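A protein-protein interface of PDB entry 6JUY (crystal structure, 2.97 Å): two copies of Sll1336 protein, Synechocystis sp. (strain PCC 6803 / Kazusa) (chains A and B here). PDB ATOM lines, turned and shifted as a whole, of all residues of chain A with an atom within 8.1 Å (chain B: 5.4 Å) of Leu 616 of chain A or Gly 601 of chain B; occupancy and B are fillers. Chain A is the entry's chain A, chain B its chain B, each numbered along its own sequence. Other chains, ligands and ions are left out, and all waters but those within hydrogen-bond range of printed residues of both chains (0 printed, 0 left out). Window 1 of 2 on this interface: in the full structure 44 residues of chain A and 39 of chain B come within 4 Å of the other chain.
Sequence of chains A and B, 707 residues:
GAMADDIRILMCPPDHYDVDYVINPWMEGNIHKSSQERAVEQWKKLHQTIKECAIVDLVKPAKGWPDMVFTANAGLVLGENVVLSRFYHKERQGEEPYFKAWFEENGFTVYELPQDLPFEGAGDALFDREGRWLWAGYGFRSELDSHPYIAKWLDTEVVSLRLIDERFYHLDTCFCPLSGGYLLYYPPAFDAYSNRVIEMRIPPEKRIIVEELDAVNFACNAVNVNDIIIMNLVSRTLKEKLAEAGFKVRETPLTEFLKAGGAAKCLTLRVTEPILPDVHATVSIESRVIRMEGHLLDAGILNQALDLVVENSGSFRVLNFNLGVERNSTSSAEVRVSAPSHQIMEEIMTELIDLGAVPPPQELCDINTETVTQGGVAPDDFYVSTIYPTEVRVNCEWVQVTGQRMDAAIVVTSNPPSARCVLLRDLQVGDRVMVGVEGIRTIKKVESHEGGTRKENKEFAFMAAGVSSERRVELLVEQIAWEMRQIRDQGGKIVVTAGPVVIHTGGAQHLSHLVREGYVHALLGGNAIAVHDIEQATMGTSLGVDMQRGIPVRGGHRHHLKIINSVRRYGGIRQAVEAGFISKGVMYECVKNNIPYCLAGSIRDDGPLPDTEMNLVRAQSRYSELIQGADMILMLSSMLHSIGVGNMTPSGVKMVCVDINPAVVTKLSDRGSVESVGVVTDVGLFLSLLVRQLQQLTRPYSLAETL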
ATOM      1  N   ARG A 425      -0.205  14.220  35.421  1.00  0.00           N
ATOM      2  CA  ARG A 425      -1.475  14.450  34.744  1.00  0.00           C
ATOM      3  C   ARG A 425      -2.477  13.336  35.034  1.00  0.00           C
ATOM      4  O   ARG A 425      -3.687  13.583  35.075  1.00  0.00           O
ATOM      5  CB  ARG A 425      -1.232  14.635  33.244  1.00  0.00           C
ATOM      6  CG  ARG A 425      -0.610  13.455  32.495  1.00  0.00           C
ATOM      7  CD  ARG A 425      -0.470  13.816  31.014  1.00  0.00           C
ATOM      8  NE  ARG A 425       0.708  13.244  30.355  1.00  0.00           N
ATOM      9  CZ  ARG A 425       0.777  12.004  29.879  1.00  0.00           C
ATOM     10  NH1 ARG A 425      -0.264  11.193  29.986  1.00  0.00           N
ATOM     11  NH2 ARG A 425       1.884  11.579  29.285  1.00  0.00           N
ATOM     12  N   LEU A 599       4.864   5.545  15.868  1.00  0.00           N
ATOM     13  CA  LEU A 599       5.497   6.691  15.228  1.00  0.00           C
ATOM     14  C   LEU A 599       4.972   7.941  15.916  1.00  0.00           C
ATOM     15  O   LEU A 599       3.836   8.361  15.684  1.00  0.00           O
ATOM     16  CB  LEU A 599       5.212   6.709  13.729  1.00  0.00           C
ATOM     17  CG  LEU A 599       5.604   5.440  12.968  1.00  0.00           C
ATOM     18  CD1 LEU A 599       5.407   5.626  11.476  1.00  0.00           C
ATOM     19  CD2 LEU A 599       7.046   5.051  13.276  1.00  0.00           C
ATOM     20  N   ALA A 600       5.808   8.527  16.766  1.00  0.00           N
ATOM     21  CA  ALA A 600       5.460   9.753  17.463  1.00  0.00           C
ATOM     22  C   ALA A 600       5.568  10.947  16.532  1.00  0.00           C
ATOM     23  O   ALA A 600       6.457  11.013  15.679  1.00  0.00           O
ATOM     24  CB  ALA A 600       6.376   9.964  18.662  1.00  0.00           C
ATOM     25  N   GLY A 601       4.666  11.902  16.709  1.00  0.00           N
ATOM     26  CA  GLY A 601       4.685  13.076  15.874  1.00  0.00           C
ATOM     27  C   GLY A 601       5.762  14.055  16.292  1.00  0.00           C
ATOM     28  O   GLY A 601       6.320  13.988  17.388  1.00  0.00           O
ATOM     29  N   SER A 602       6.053  14.987  15.391  1.00  0.00           N
ATOM     30  CA  SER A 602       7.008  16.053  15.646  1.00  0.00           C
ATOM     31  C   SER A 602       6.474  17.332  15.027  1.00  0.00           C
ATOM     32  O   SER A 602       5.668  17.295  14.095  1.00  0.00           O
ATOM     33  CB  SER A 602       8.391  15.716  15.073  1.00  0.00           C
ATOM     34  OG  SER A 602       9.188  16.877  14.937  1.00  0.00           O
ATOM     35  N   ILE A 603       6.915  18.472  15.564  1.00  0.00           N
ATOM     36  CA  ILE A 603       6.477  19.744  15.004  1.00  0.00           C
ATOM     37  C   ILE A 603       7.009  19.930  13.589  1.00  0.00           C
ATOM     38  O   ILE A 603       6.455  20.725  12.818  1.00  0.00           O
ATOM     39  CB  ILE A 603       6.879  20.912  15.925  1.00  0.00           C
ATOM     40  CG1 ILE A 603       6.061  22.155  15.575  1.00  0.00           C
ATOM     41  CG2 ILE A 603       8.369  21.206  15.811  1.00  0.00           C
ATOM     42  CD1 ILE A 603       4.575  21.997  15.849  1.00  0.00           C
ATOM     43  N   ARG A 604       8.076  19.217  13.228  1.00  0.00           N
ATOM     44  CA  ARG A 604       8.658  19.262  11.892  1.00  0.00           C
ATOM     45  C   ARG A 604       7.976  18.319  10.906  1.00  0.00           C
ATOM     46  O   ARG A 604       8.330  18.334   9.721  1.00  0.00           O
ATOM     47  CB  ARG A 604      10.154  18.942  11.968  1.00  0.00           C
ATOM     48  N   ASP A 605       7.018  17.509  11.358  1.00  0.00           N
ATOM     49  CA  ASP A 605       6.478  16.433  10.530  1.00  0.00           C
ATOM     50  C   ASP A 605       5.740  16.979   9.314  1.00  0.00           C
ATOM     51  O   ASP A 605       4.840  17.815   9.434  1.00  0.00           O
ATOM     52  CB  ASP A 605       5.562  15.535  11.362  1.00  0.00           C
ATOM     53  CG  ASP A 605       6.344  14.583  12.241  1.00  0.00           C
ATOM     54  OD1 ASP A 605       7.589  14.667  12.222  1.00  0.00           O
ATOM     55  OD2 ASP A 605       5.728  13.761  12.953  1.00  0.00           O
ATOM     56  N   THR A 612       1.347   8.012  11.967  1.00  0.00           N
ATOM     57  CA  THR A 612       2.041   8.893  12.899  1.00  0.00           C
ATOM     58  C   THR A 612       1.053   9.494  13.890  1.00  0.00           C
ATOM     59  O   THR A 612       0.111  10.193  13.499  1.00  0.00           O
ATOM     60  CB  THR A 612       2.768   9.998  12.133  1.00  0.00           C
ATOM     61  OG1 THR A 612       3.778   9.422  11.295  1.00  0.00           O
ATOM     62  CG2 THR A 612       3.414  10.985  13.095  1.00  0.00           C
ATOM     63  N   GLU A 613       1.275   9.221  15.175  1.00  0.00           N
ATOM     64  CA  GLU A 613       0.392   9.680  16.241  1.00  0.00           C
ATOM     65  C   GLU A 613       0.672  11.151  16.521  1.00  0.00           C
ATOM     66  O   GLU A 613       1.721  11.496  17.075  1.00  0.00           O
ATOM     67  CB  GLU A 613       0.580   8.829  17.492  1.00  0.00           C
ATOM     68  CG  GLU A 613      -0.219   9.325  18.672  1.00  0.00           C
ATOM     69  CD  GLU A 613      -1.703   9.338  18.377  1.00  0.00           C
ATOM     70  OE1 GLU A 613      -2.255   8.272  18.037  1.00  0.00           O
ATOM     71  OE2 GLU A 613      -2.313  10.422  18.465  1.00  0.00           O
ATOM     72  N   MET A 614      -0.262  12.021  16.147  1.00  0.00           N
ATOM     73  CA  MET A 614      -0.092  13.454  16.340  1.00  0.00           C
ATOM     74  C   MET A 614      -0.604  13.942  17.691  1.00  0.00           C
ATOM     75  O   MET A 614      -0.440  15.126  18.003  1.00  0.00           O
ATOM     76  CB  MET A 614      -0.776  14.226  15.209  1.00  0.00           C
ATOM     77  CG  MET A 614      -0.216  13.905  13.829  1.00  0.00           C
ATOM     78  SD  MET A 614       1.550  14.242  13.667  1.00  0.00           S
ATOM     79  CE  MET A 614       1.552  16.012  13.404  1.00  0.00           C
ATOM     80  N   ASN A 615      -1.214  13.073  18.495  1.00  0.00           N
ATOM     81  CA  ASN A 615      -1.609  13.407  19.860  1.00  0.00           C
ATOM     82  C   ASN A 615      -0.595  12.775  20.804  1.00  0.00           C
ATOM     83  O   ASN A 615      -0.587  11.556  20.999  1.00  0.00           O
ATOM     84  CB  ASN A 615      -3.029  12.925  20.156  1.00  0.00           C
ATOM     85  CG  ASN A 615      -3.395  13.041  21.625  1.00  0.00           C
ATOM     86  OD1 ASN A 615      -3.987  12.127  22.200  1.00  0.00           O
ATOM     87  ND2 ASN A 615      -3.033  14.158  22.242  1.00  0.00           N
ATOM     88  N   LEU A 616       0.258  13.614  21.394  1.00  0.00           N
ATOM     89  CA  LEU A 616       1.456  13.125  22.062  1.00  0.00           C
ATOM     90  C   LEU A 616       1.186  12.549  23.443  1.00  0.00           C
ATOM     91  O   LEU A 616       2.035  11.823  23.961  1.00  0.00           O
ATOM     92  CB  LEU A 616       2.497  14.237  22.165  1.00  0.00           C
ATOM     93  CG  LEU A 616       3.159  14.625  20.846  1.00  0.00           C
ATOM     94  CD1 LEU A 616       3.865  15.946  21.022  1.00  0.00           C
ATOM     95  CD2 LEU A 616       4.123  13.544  20.381  1.00  0.00           C
ATOM     96  N   VAL A 617       0.043  12.857  24.058  1.00  0.00           N
ATOM     97  CA  VAL A 617      -0.323  12.153  25.283  1.00  0.00           C
ATOM     98  C   VAL A 617      -0.617  10.692  24.970  1.00  0.00           C
ATOM     99  O   VAL A 617      -0.152   9.778  25.667  1.00  0.00           O
ATOM    100  CB  VAL A 617      -1.521  12.844  25.959  1.00  0.00           C
ATOM    101  N   ARG A 618      -1.374  10.452  23.899  1.00  0.00           N
ATOM    102  CA  ARG A 618      -1.598   9.092  23.425  1.00  0.00           C
ATOM    103  C   ARG A 618      -0.284   8.430  23.038  1.00  0.00           C
ATOM    104  O   ARG A 618      -0.077   7.240  23.301  1.00  0.00           O
ATOM    105  CB  ARG A 618      -2.567   9.108  22.243  1.00  0.00           C
ATOM    106  CG  ARG A 618      -2.985   7.734  21.759  1.00  0.00           C
ATOM    107  CD  ARG A 618      -4.012   7.850  20.648  1.00  0.00           C
ATOM    108  NE  ARG A 618      -5.061   8.806  20.985  1.00  0.00           N
ATOM    109  CZ  ARG A 618      -6.073   9.121  20.184  1.00  0.00           C
ATOM    110  NH1 ARG A 618      -6.179   8.552  18.991  1.00  0.00           N
ATOM    111  NH2 ARG A 618      -6.980  10.005  20.577  1.00  0.00           N
ATOM    112  N   ALA A 619       0.614   9.187  22.402  1.00  0.00           N
ATOM    113  CA  ALA A 619       1.900   8.626  22.004  1.00  0.00           C
ATOM    114  C   ALA A 619       2.734   8.239  23.218  1.00  0.00           C
ATOM    115  O   ALA A 619       3.386   7.193  23.213  1.00  0.00           O
ATOM    116  CB  ALA A 619       2.658   9.618  21.122  1.00  0.00           C
ATOM    117  N   GLN A 620       2.737   9.072  24.261  1.00  0.00           N
ATOM    118  CA  GLN A 620       3.467   8.735  25.480  1.00  0.00           C
ATOM    119  C   GLN A 620       2.869   7.509  26.162  1.00  0.00           C
ATOM    120  O   GLN A 620       3.603   6.645  26.661  1.00  0.00           O
ATOM    121  CB  GLN A 620       3.480   9.943  26.420  1.00  0.00           C
ATOM    122  CG  GLN A 620       4.488  11.011  26.011  1.00  0.00           C
ATOM    123  CD  GLN A 620       4.553  12.173  26.984  1.00  0.00           C
ATOM    124  OE1 GLN A 620       3.824  12.215  27.973  1.00  0.00           O
ATOM    125  NE2 GLN A 620       5.437  13.124  26.705  1.00  0.00           N
ATOM    126  N   SER A 621       1.537   7.408  26.180  1.00  0.00           N
ATOM    127  CA  SER A 621       0.897   6.222  26.744  1.00  0.00           C
ATOM    128  C   SER A 621       1.297   4.967  25.976  1.00  0.00           C
ATOM    129  O   SER A 621       1.682   3.953  26.570  1.00  0.00           O
ATOM    130  CB  SER A 621      -0.622   6.395  26.745  1.00  0.00           C
ATOM    131  OG  SER A 621      -1.006   7.555  27.461  1.00  0.00           O
ATOM    132  N   ARG A 622       1.209   5.020  24.646  1.00  0.00           N
ATOM    133  CA  ARG A 622       1.577   3.874  23.819  1.00  0.00           C
ATOM    134  C   ARG A 622       3.061   3.539  23.949  1.00  0.00           C
ATOM    135  O   ARG A 622       3.445   2.362  23.929  1.00  0.00           O
ATOM    136  CB  ARG A 622       1.199   4.161  22.368  1.00  0.00           C
ATOM    137  CG  ARG A 622       1.506   3.046  21.393  1.00  0.00           C
ATOM    138  CD  ARG A 622       0.685   1.807  21.660  1.00  0.00           C
ATOM    139  NE  ARG A 622       0.934   0.768  20.663  1.00  0.00           N
ATOM    140  CZ  ARG A 622       0.695  -0.526  20.843  1.00  0.00           C
ATOM    141  NH1 ARG A 622       0.201  -0.963  21.992  1.00  0.00           N
ATOM    142  NH2 ARG A 622       0.943  -1.384  19.862  1.00  0.00           N
ATOM    143  N   TYR A 623       3.913   4.560  24.077  1.00  0.00           N
ATOM    144  CA  TYR A 623       5.339   4.339  24.298  1.00  0.00           C
ATOM    145  C   TYR A 623       5.577   3.581  25.597  1.00  0.00           C
ATOM    146  O   TYR A 623       6.356   2.622  25.635  1.00  0.00           O
ATOM    147  CB  TYR A 623       6.073   5.683  24.303  1.00  0.00           C
ATOM    148  CG  TYR A 623       6.725   6.032  22.981  1.00  0.00           C
ATOM    149  CD1 TYR A 623       5.992   6.036  21.802  1.00  0.00           C
ATOM    150  CD2 TYR A 623       8.073   6.362  22.915  1.00  0.00           C
ATOM    151  CE1 TYR A 623       6.585   6.353  20.592  1.00  0.00           C
ATOM    152  CE2 TYR A 623       8.673   6.681  21.710  1.00  0.00           C
ATOM    153  CZ  TYR A 623       7.926   6.676  20.553  1.00  0.00           C
ATOM    154  OH  TYR A 623       8.518   6.995  19.352  1.00  0.00           O
ATOM    155  N   LEU A 640      16.267  13.684  21.508  1.00  0.00           N
ATOM    156  CA  LEU A 640      14.894  13.972  21.916  1.00  0.00           C
ATOM    157  C   LEU A 640      14.058  12.704  21.997  1.00  0.00           C
ATOM    158  O   LEU A 640      13.340  12.479  22.978  1.00  0.00           O
ATOM    159  CB  LEU A 640      14.271  14.969  20.935  1.00  0.00           C
ATOM    160  CG  LEU A 640      12.764  15.222  20.991  1.00  0.00           C
ATOM    161  CD1 LEU A 640      12.403  16.073  22.197  1.00  0.00           C
ATOM    162  CD2 LEU A 640      12.284  15.872  19.700  1.00  0.00           C
ATOM    163  N   MET A 648      10.946   7.138  30.150  1.00  0.00           N
ATOM    164  CA  MET A 648       9.871   6.190  30.432  1.00  0.00           C
ATOM    165  C   MET A 648      10.353   4.844  30.979  1.00  0.00           C
ATOM    166  O   MET A 648       9.540   4.108  31.549  1.00  0.00           O
ATOM    167  CB  MET A 648       9.026   5.980  29.173  1.00  0.00           C
ATOM    168  CG  MET A 648       8.048   7.118  28.905  1.00  0.00           C
ATOM    169  SD  MET A 648       7.603   7.286  27.166  1.00  0.00           S
ATOM    170  N   LEU B 599       3.815  26.831  22.378  1.00  0.00           N
ATOM    171  CA  LEU B 599       4.683  25.777  22.890  1.00  0.00           C
ATOM    172  C   LEU B 599       4.244  24.472  22.239  1.00  0.00           C
ATOM    173  O   LEU B 599       3.234  23.879  22.627  1.00  0.00           O
ATOM    174  CB  LEU B 599       4.598  25.696  24.410  1.00  0.00           C
ATOM    175  CG  LEU B 599       4.863  26.978  25.202  1.00  0.00           C
ATOM    176  CD1 LEU B 599       4.870  26.688  26.693  1.00  0.00           C
ATOM    177  CD2 LEU B 599       6.169  27.625  24.772  1.00  0.00           C
ATOM    178  N   ALA B 600       5.006  24.023  21.250  1.00  0.00           N
ATOM    179  CA  ALA B 600       4.726  22.753  20.607  1.00  0.00           C
ATOM    180  C   ALA B 600       5.195  21.616  21.498  1.00  0.00           C
ATOM    181  O   ALA B 600       6.246  21.701  22.140  1.00  0.00           O
ATOM    182  CB  ALA B 600       5.415  22.677  19.246  1.00  0.00           C
ATOM    183  N   GLY B 601       4.411  20.550  21.536  1.00  0.00           N
ATOM    184  CA  GLY B 601       4.758  19.421  22.361  1.00  0.00           C
ATOM    185  C   GLY B 601       5.799  18.525  21.721  1.00  0.00           C
ATOM    186  O   GLY B 601       6.064  18.578  20.520  1.00  0.00           O
ATOM    187  N   SER B 602       6.395  17.684  22.558  1.00  0.00           N
ATOM    188  CA  SER B 602       7.343  16.673  22.123  1.00  0.00           C
ATOM    189  C   SER B 602       7.096  15.425  22.953  1.00  0.00           C
ATOM    190  O   SER B 602       6.539  15.493  24.051  1.00  0.00           O
ATOM    191  CB  SER B 602       8.798  17.139  22.268  1.00  0.00           C
ATOM    192  OG  SER B 602       9.149  17.317  23.629  1.00  0.00           O
ATOM    193  N   ILE B 603       7.509  14.273  22.422  1.00  0.00           N
ATOM    194  CA  ILE B 603       7.329  13.032  23.164  1.00  0.00           C
ATOM    195  C   ILE B 603       8.137  13.008  24.458  1.00  0.00           C
ATOM    196  O   ILE B 603       7.818  12.239  25.372  1.00  0.00           O
ATOM    197  CB  ILE B 603       7.659  11.814  22.282  1.00  0.00           C
ATOM    198  CG1 ILE B 603       7.125  10.548  22.954  1.00  0.00           C
ATOM    199  CG2 ILE B 603       9.155  11.728  22.014  1.00  0.00           C
ATOM    200  CD1 ILE B 603       6.683   9.495  22.021  1.00  0.00           C
ATOM    201  N   ASP B 605       8.202  15.394  26.605  1.00  0.00           N
ATOM    202  CA  ASP B 605       7.650  16.401  27.506  1.00  0.00           C
ATOM    203  C   ASP B 605       7.170  15.807  28.830  1.00  0.00           C
ATOM    204  O   ASP B 605       6.387  14.854  28.846  1.00  0.00           O
ATOM    205  CB  ASP B 605       6.488  17.123  26.822  1.00  0.00           C
ATOM    206  CG  ASP B 605       6.952  18.122  25.788  1.00  0.00           C
ATOM    207  OD1 ASP B 605       8.173  18.212  25.551  1.00  0.00           O
ATOM    208  OD2 ASP B 605       6.094  18.827  25.216  1.00  0.00           O
ATOM    209  N   THR B 612       1.337  24.008  26.748  1.00  0.00           N
ATOM    210  CA  THR B 612       1.959  23.340  25.610  1.00  0.00           C
ATOM    211  C   THR B 612       0.942  22.500  24.844  1.00  0.00           C
ATOM    212  O   THR B 612       0.271  21.638  25.421  1.00  0.00           O
ATOM    213  CB  THR B 612       3.125  22.475  26.074  1.00  0.00           C
ATOM    214  OG1 THR B 612       2.629  21.227  26.565  1.00  0.00           O
ATOM    215  CG2 THR B 612       3.891  23.182  27.173  1.00  0.00           C
ATOM    216  N   GLU B 613       0.826  22.764  23.545  1.00  0.00           N
ATOM    217  CA  GLU B 613      -0.122  22.071  22.678  1.00  0.00           C
ATOM    218  C   GLU B 613       0.411  20.673  22.375  1.00  0.00           C
ATOM    219  O   GLU B 613       1.364  20.520  21.604  1.00  0.00           O
ATOM    220  CB  GLU B 613      -0.343  22.875  21.401  1.00  0.00           C
ATOM    221  CG  GLU B 613      -1.212  22.190  20.369  1.00  0.00           C
ATOM    222  CD  GLU B 613      -2.603  21.898  20.886  1.00  0.00           C
ATOM    223  OE1 GLU B 613      -3.292  22.851  21.307  1.00  0.00           O
ATOM    224  OE2 GLU B 613      -3.010  20.719  20.864  1.00  0.00           O
ATOM    225  N   MET B 614      -0.204  19.650  22.973  1.00  0.00           N
ATOM    226  CA  MET B 614       0.237  18.273  22.781  1.00  0.00           C
ATOM    227  C   MET B 614      -0.323  17.617  21.526  1.00  0.00           C
ATOM    228  O   MET B 614       0.072  16.486  21.217  1.00  0.00           O
ATOM    229  CB  MET B 614      -0.132  17.421  23.997  1.00  0.00           C
ATOM    230  CG  MET B 614       0.533  17.867  25.279  1.00  0.00           C
ATOM    231  SD  MET B 614       2.329  17.811  25.137  1.00  0.00           S
ATOM    232  CE  MET B 614       2.633  16.065  25.395  1.00  0.00           C
ATOM    233  N   ASN B 615      -1.222  18.278  20.802  1.00  0.00           N
ATOM    234  CA  ASN B 615      -1.720  17.777  19.524  1.00  0.00           C
ATOM    235  C   ASN B 615      -1.032  18.578  18.425  1.00  0.00           C
ATOM    236  O   ASN B 615      -1.312  19.767  18.246  1.00  0.00           O
ATOM    237  CB  ASN B 615      -3.238  17.896  19.437  1.00  0.00           C
ATOM    238  CG  ASN B 615      -3.775  17.518  18.071  1.00  0.00           C
ATOM    239  OD1 ASN B 615      -4.066  18.381  17.240  1.00  0.00           O
ATOM    240  ND2 ASN B 615      -3.923  16.220  17.838  1.00  0.00           N
ATOM    241  N   LEU B 616      -0.128  17.925  17.691  1.00  0.00           N
ATOM    242  CA  LEU B 616       0.830  18.647  16.860  1.00  0.00           C
ATOM    243  C   LEU B 616       0.249  19.188  15.561  1.00  0.00           C
ATOM    244  O   LEU B 616       0.875  20.056  14.949  1.00  0.00           O
ATOM    245  CB  LEU B 616       2.033  17.761  16.549  1.00  0.00           C
ATOM    246  CG  LEU B 616       2.929  17.562  17.766  1.00  0.00           C
ATOM    247  CD1 LEU B 616       3.869  16.414  17.530  1.00  0.00           C
ATOM    248  CD2 LEU B 616       3.699  18.840  18.060  1.00  0.00           C
ATOM    249  N   ALA B 619      -0.715  22.457  16.851  1.00  0.00           N
ATOM    250  CA  ALA B 619       0.501  23.228  17.085  1.00  0.00           C
ATOM    251  C   ALA B 619       1.097  23.735  15.778  1.00  0.00           C
ATOM    252  O   ALA B 619       1.563  24.878  15.708  1.00  0.00           O
ATOM    253  CB  ALA B 619       1.514  22.381  17.853  1.00  0.00           C
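O of Met 614 of chain A is in hydrogen-bond range of N of Leu 616 of chain B (2.8 Å). The backbone NH of Leu 616 of chain A is in hydrogen-bond range of the backbone carbonyl oxygen of Met 614 of chain B (2.9 Å). NE2 of Gln 620 of chain A is in hydrogen-bond range of O of Ile 603 of chain B, 2.9 Å away. The side-chain amide nitrogen (NE2) of Gln 620 of chain A sits at hydrogen-bond distance from the backbone carbonyl oxygen (O) of Asp 605 of chain B (2.9 Å).
The side-chain carboxylate (OE2) of Glu 613 of chain A sits at hydrogen-bond distance from the backbone NH (N) of Asn 615 of chain A (2.9 Å). The side-chain hydroxyl of Ser 602 of chain A sits close to the backbone NH of Arg 604 of chain A, 3.1 Å away. The guanidinium group (NH2) of Arg 425 of chain A is in hydrogen-bond range of the side-chain amide oxygen (OE1) of Gln 620 of chain A, at 2.4 Å. The backbone NH of Ser 602 of chain B is in hydrogen-bond range of the side-chain carboxylate of Asp 605 of chain B, at 2.9 Å. OE2 of Glu 613 of chain B lies within hydrogen-bond range of N of Asn 615 of chain B (3.0 Å). The backbone NH of Gly 601 of chain A is in hydrogen-bond range of the backbone carbonyl oxygen of Glu 613 of chain A (3.0 Å).
Among the printed residues, merely in contact across the chains: Ala 600 of chain A with Ile 603 of chain B (3.4 Å), Gly 601 of chain A with Leu 616 of chain B (3.3 Å), Ser 602 of chain A with Leu 616 of chain B (3.4 Å), Ile 603 of chain A with Ala 600 of chain B (3.6 Å), Ile 603 of chain A with Leu 616 of chain B (3.95 Å), Ile 603 of chain A with Ala 619 of chain B (3.7 Å), Met 614 of chain A with Met 614 of chain B (3.5 Å), Met 614 of chain A with Asn 615 of chain B (3.3 Å), Asn 615 of chain A with Met 614 of chain B (3.8 Å), Leu 616 of chain A with Gly 601 of chain B (3.3 Å), Leu 616 of chain A with Ser 602 of chain B (3.4 Å), Leu 616 of chain A with Leu 616 of chain B (3.5 Å), Gln 620 of chain A with Ser 602 of chain B (3.7 Å), Tyr 623 of chain A with Ile 603 of chain B (3.4 Å) and Leu 640 of chain A with Ser 602 of chain B (3.8 Å).
Of chain B, only Gly 601 (3.3 Å), Ser 602 (3.4 Å), Met 614 (2.9 Å) and Leu 616 (3.5 Å) come within 4 Å of Leu 616 of chain A. Gly 601 of chain B touches just one residue of chain A: Leu 616. Ala 600 of chain B touches just one residue of chain A: Ile 603 (3.6 Å). Printed residues of chain A within 4 Å of Ser 602 of chain B: Leu 616, Gln 620 and Leu 640. Of the printed residues of chain B, Tyr 623 of chain A touches Ile 603 (3.4 Å). Of the printed residues of chain A, Asp 605 of chain B touches Gln 620 (2.9 Å). Leu 599 of chain A touches none of the printed residues of chain B. The nearest residue of chain B that does not touch Leu 616 of chain A is Ile 603 of chain B (4.02 Å). The nearest residue of chain A that does not touch Gly 601 of chain B is Ile 603 of chain A (5.0 Å). The nearest printed residue of chain B that does not touch Ala 600 of chain A is Leu 616 of chain B (5.8 Å).
Of the 22 printed residues of chain A, 10 touch a printed residue of chain B. Of the 12 printed residues of chain B, 9 touch a printed residue of chain A. Hydrophobic or aromatic side chains of chain B that line the printed part of chain A: Ala 600, Ile 603, Met 614, Leu 616 and Ala 619. Among the printed residues, 19 pairs touch across the chains.
Ile 603 of chain A touches Leu 616 of chain B, but with the chains exchanged Leu 616 of chain A does not touch Ile 603 of chain B (4.02 Å). Ile 603 of chain A touches Ala 619 of chain B, but with the chains exchanged Ala 619 of chain A does not touch Ile 603 of chain B (4.1 Å). Met 614 of chain B touches its own counterpart, Met 614 of chain A. Met 614 of chain A touches Asn 615 of chain B, and with the chains exchanged Asn 615 of chain A touches Met 614 of chain B.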
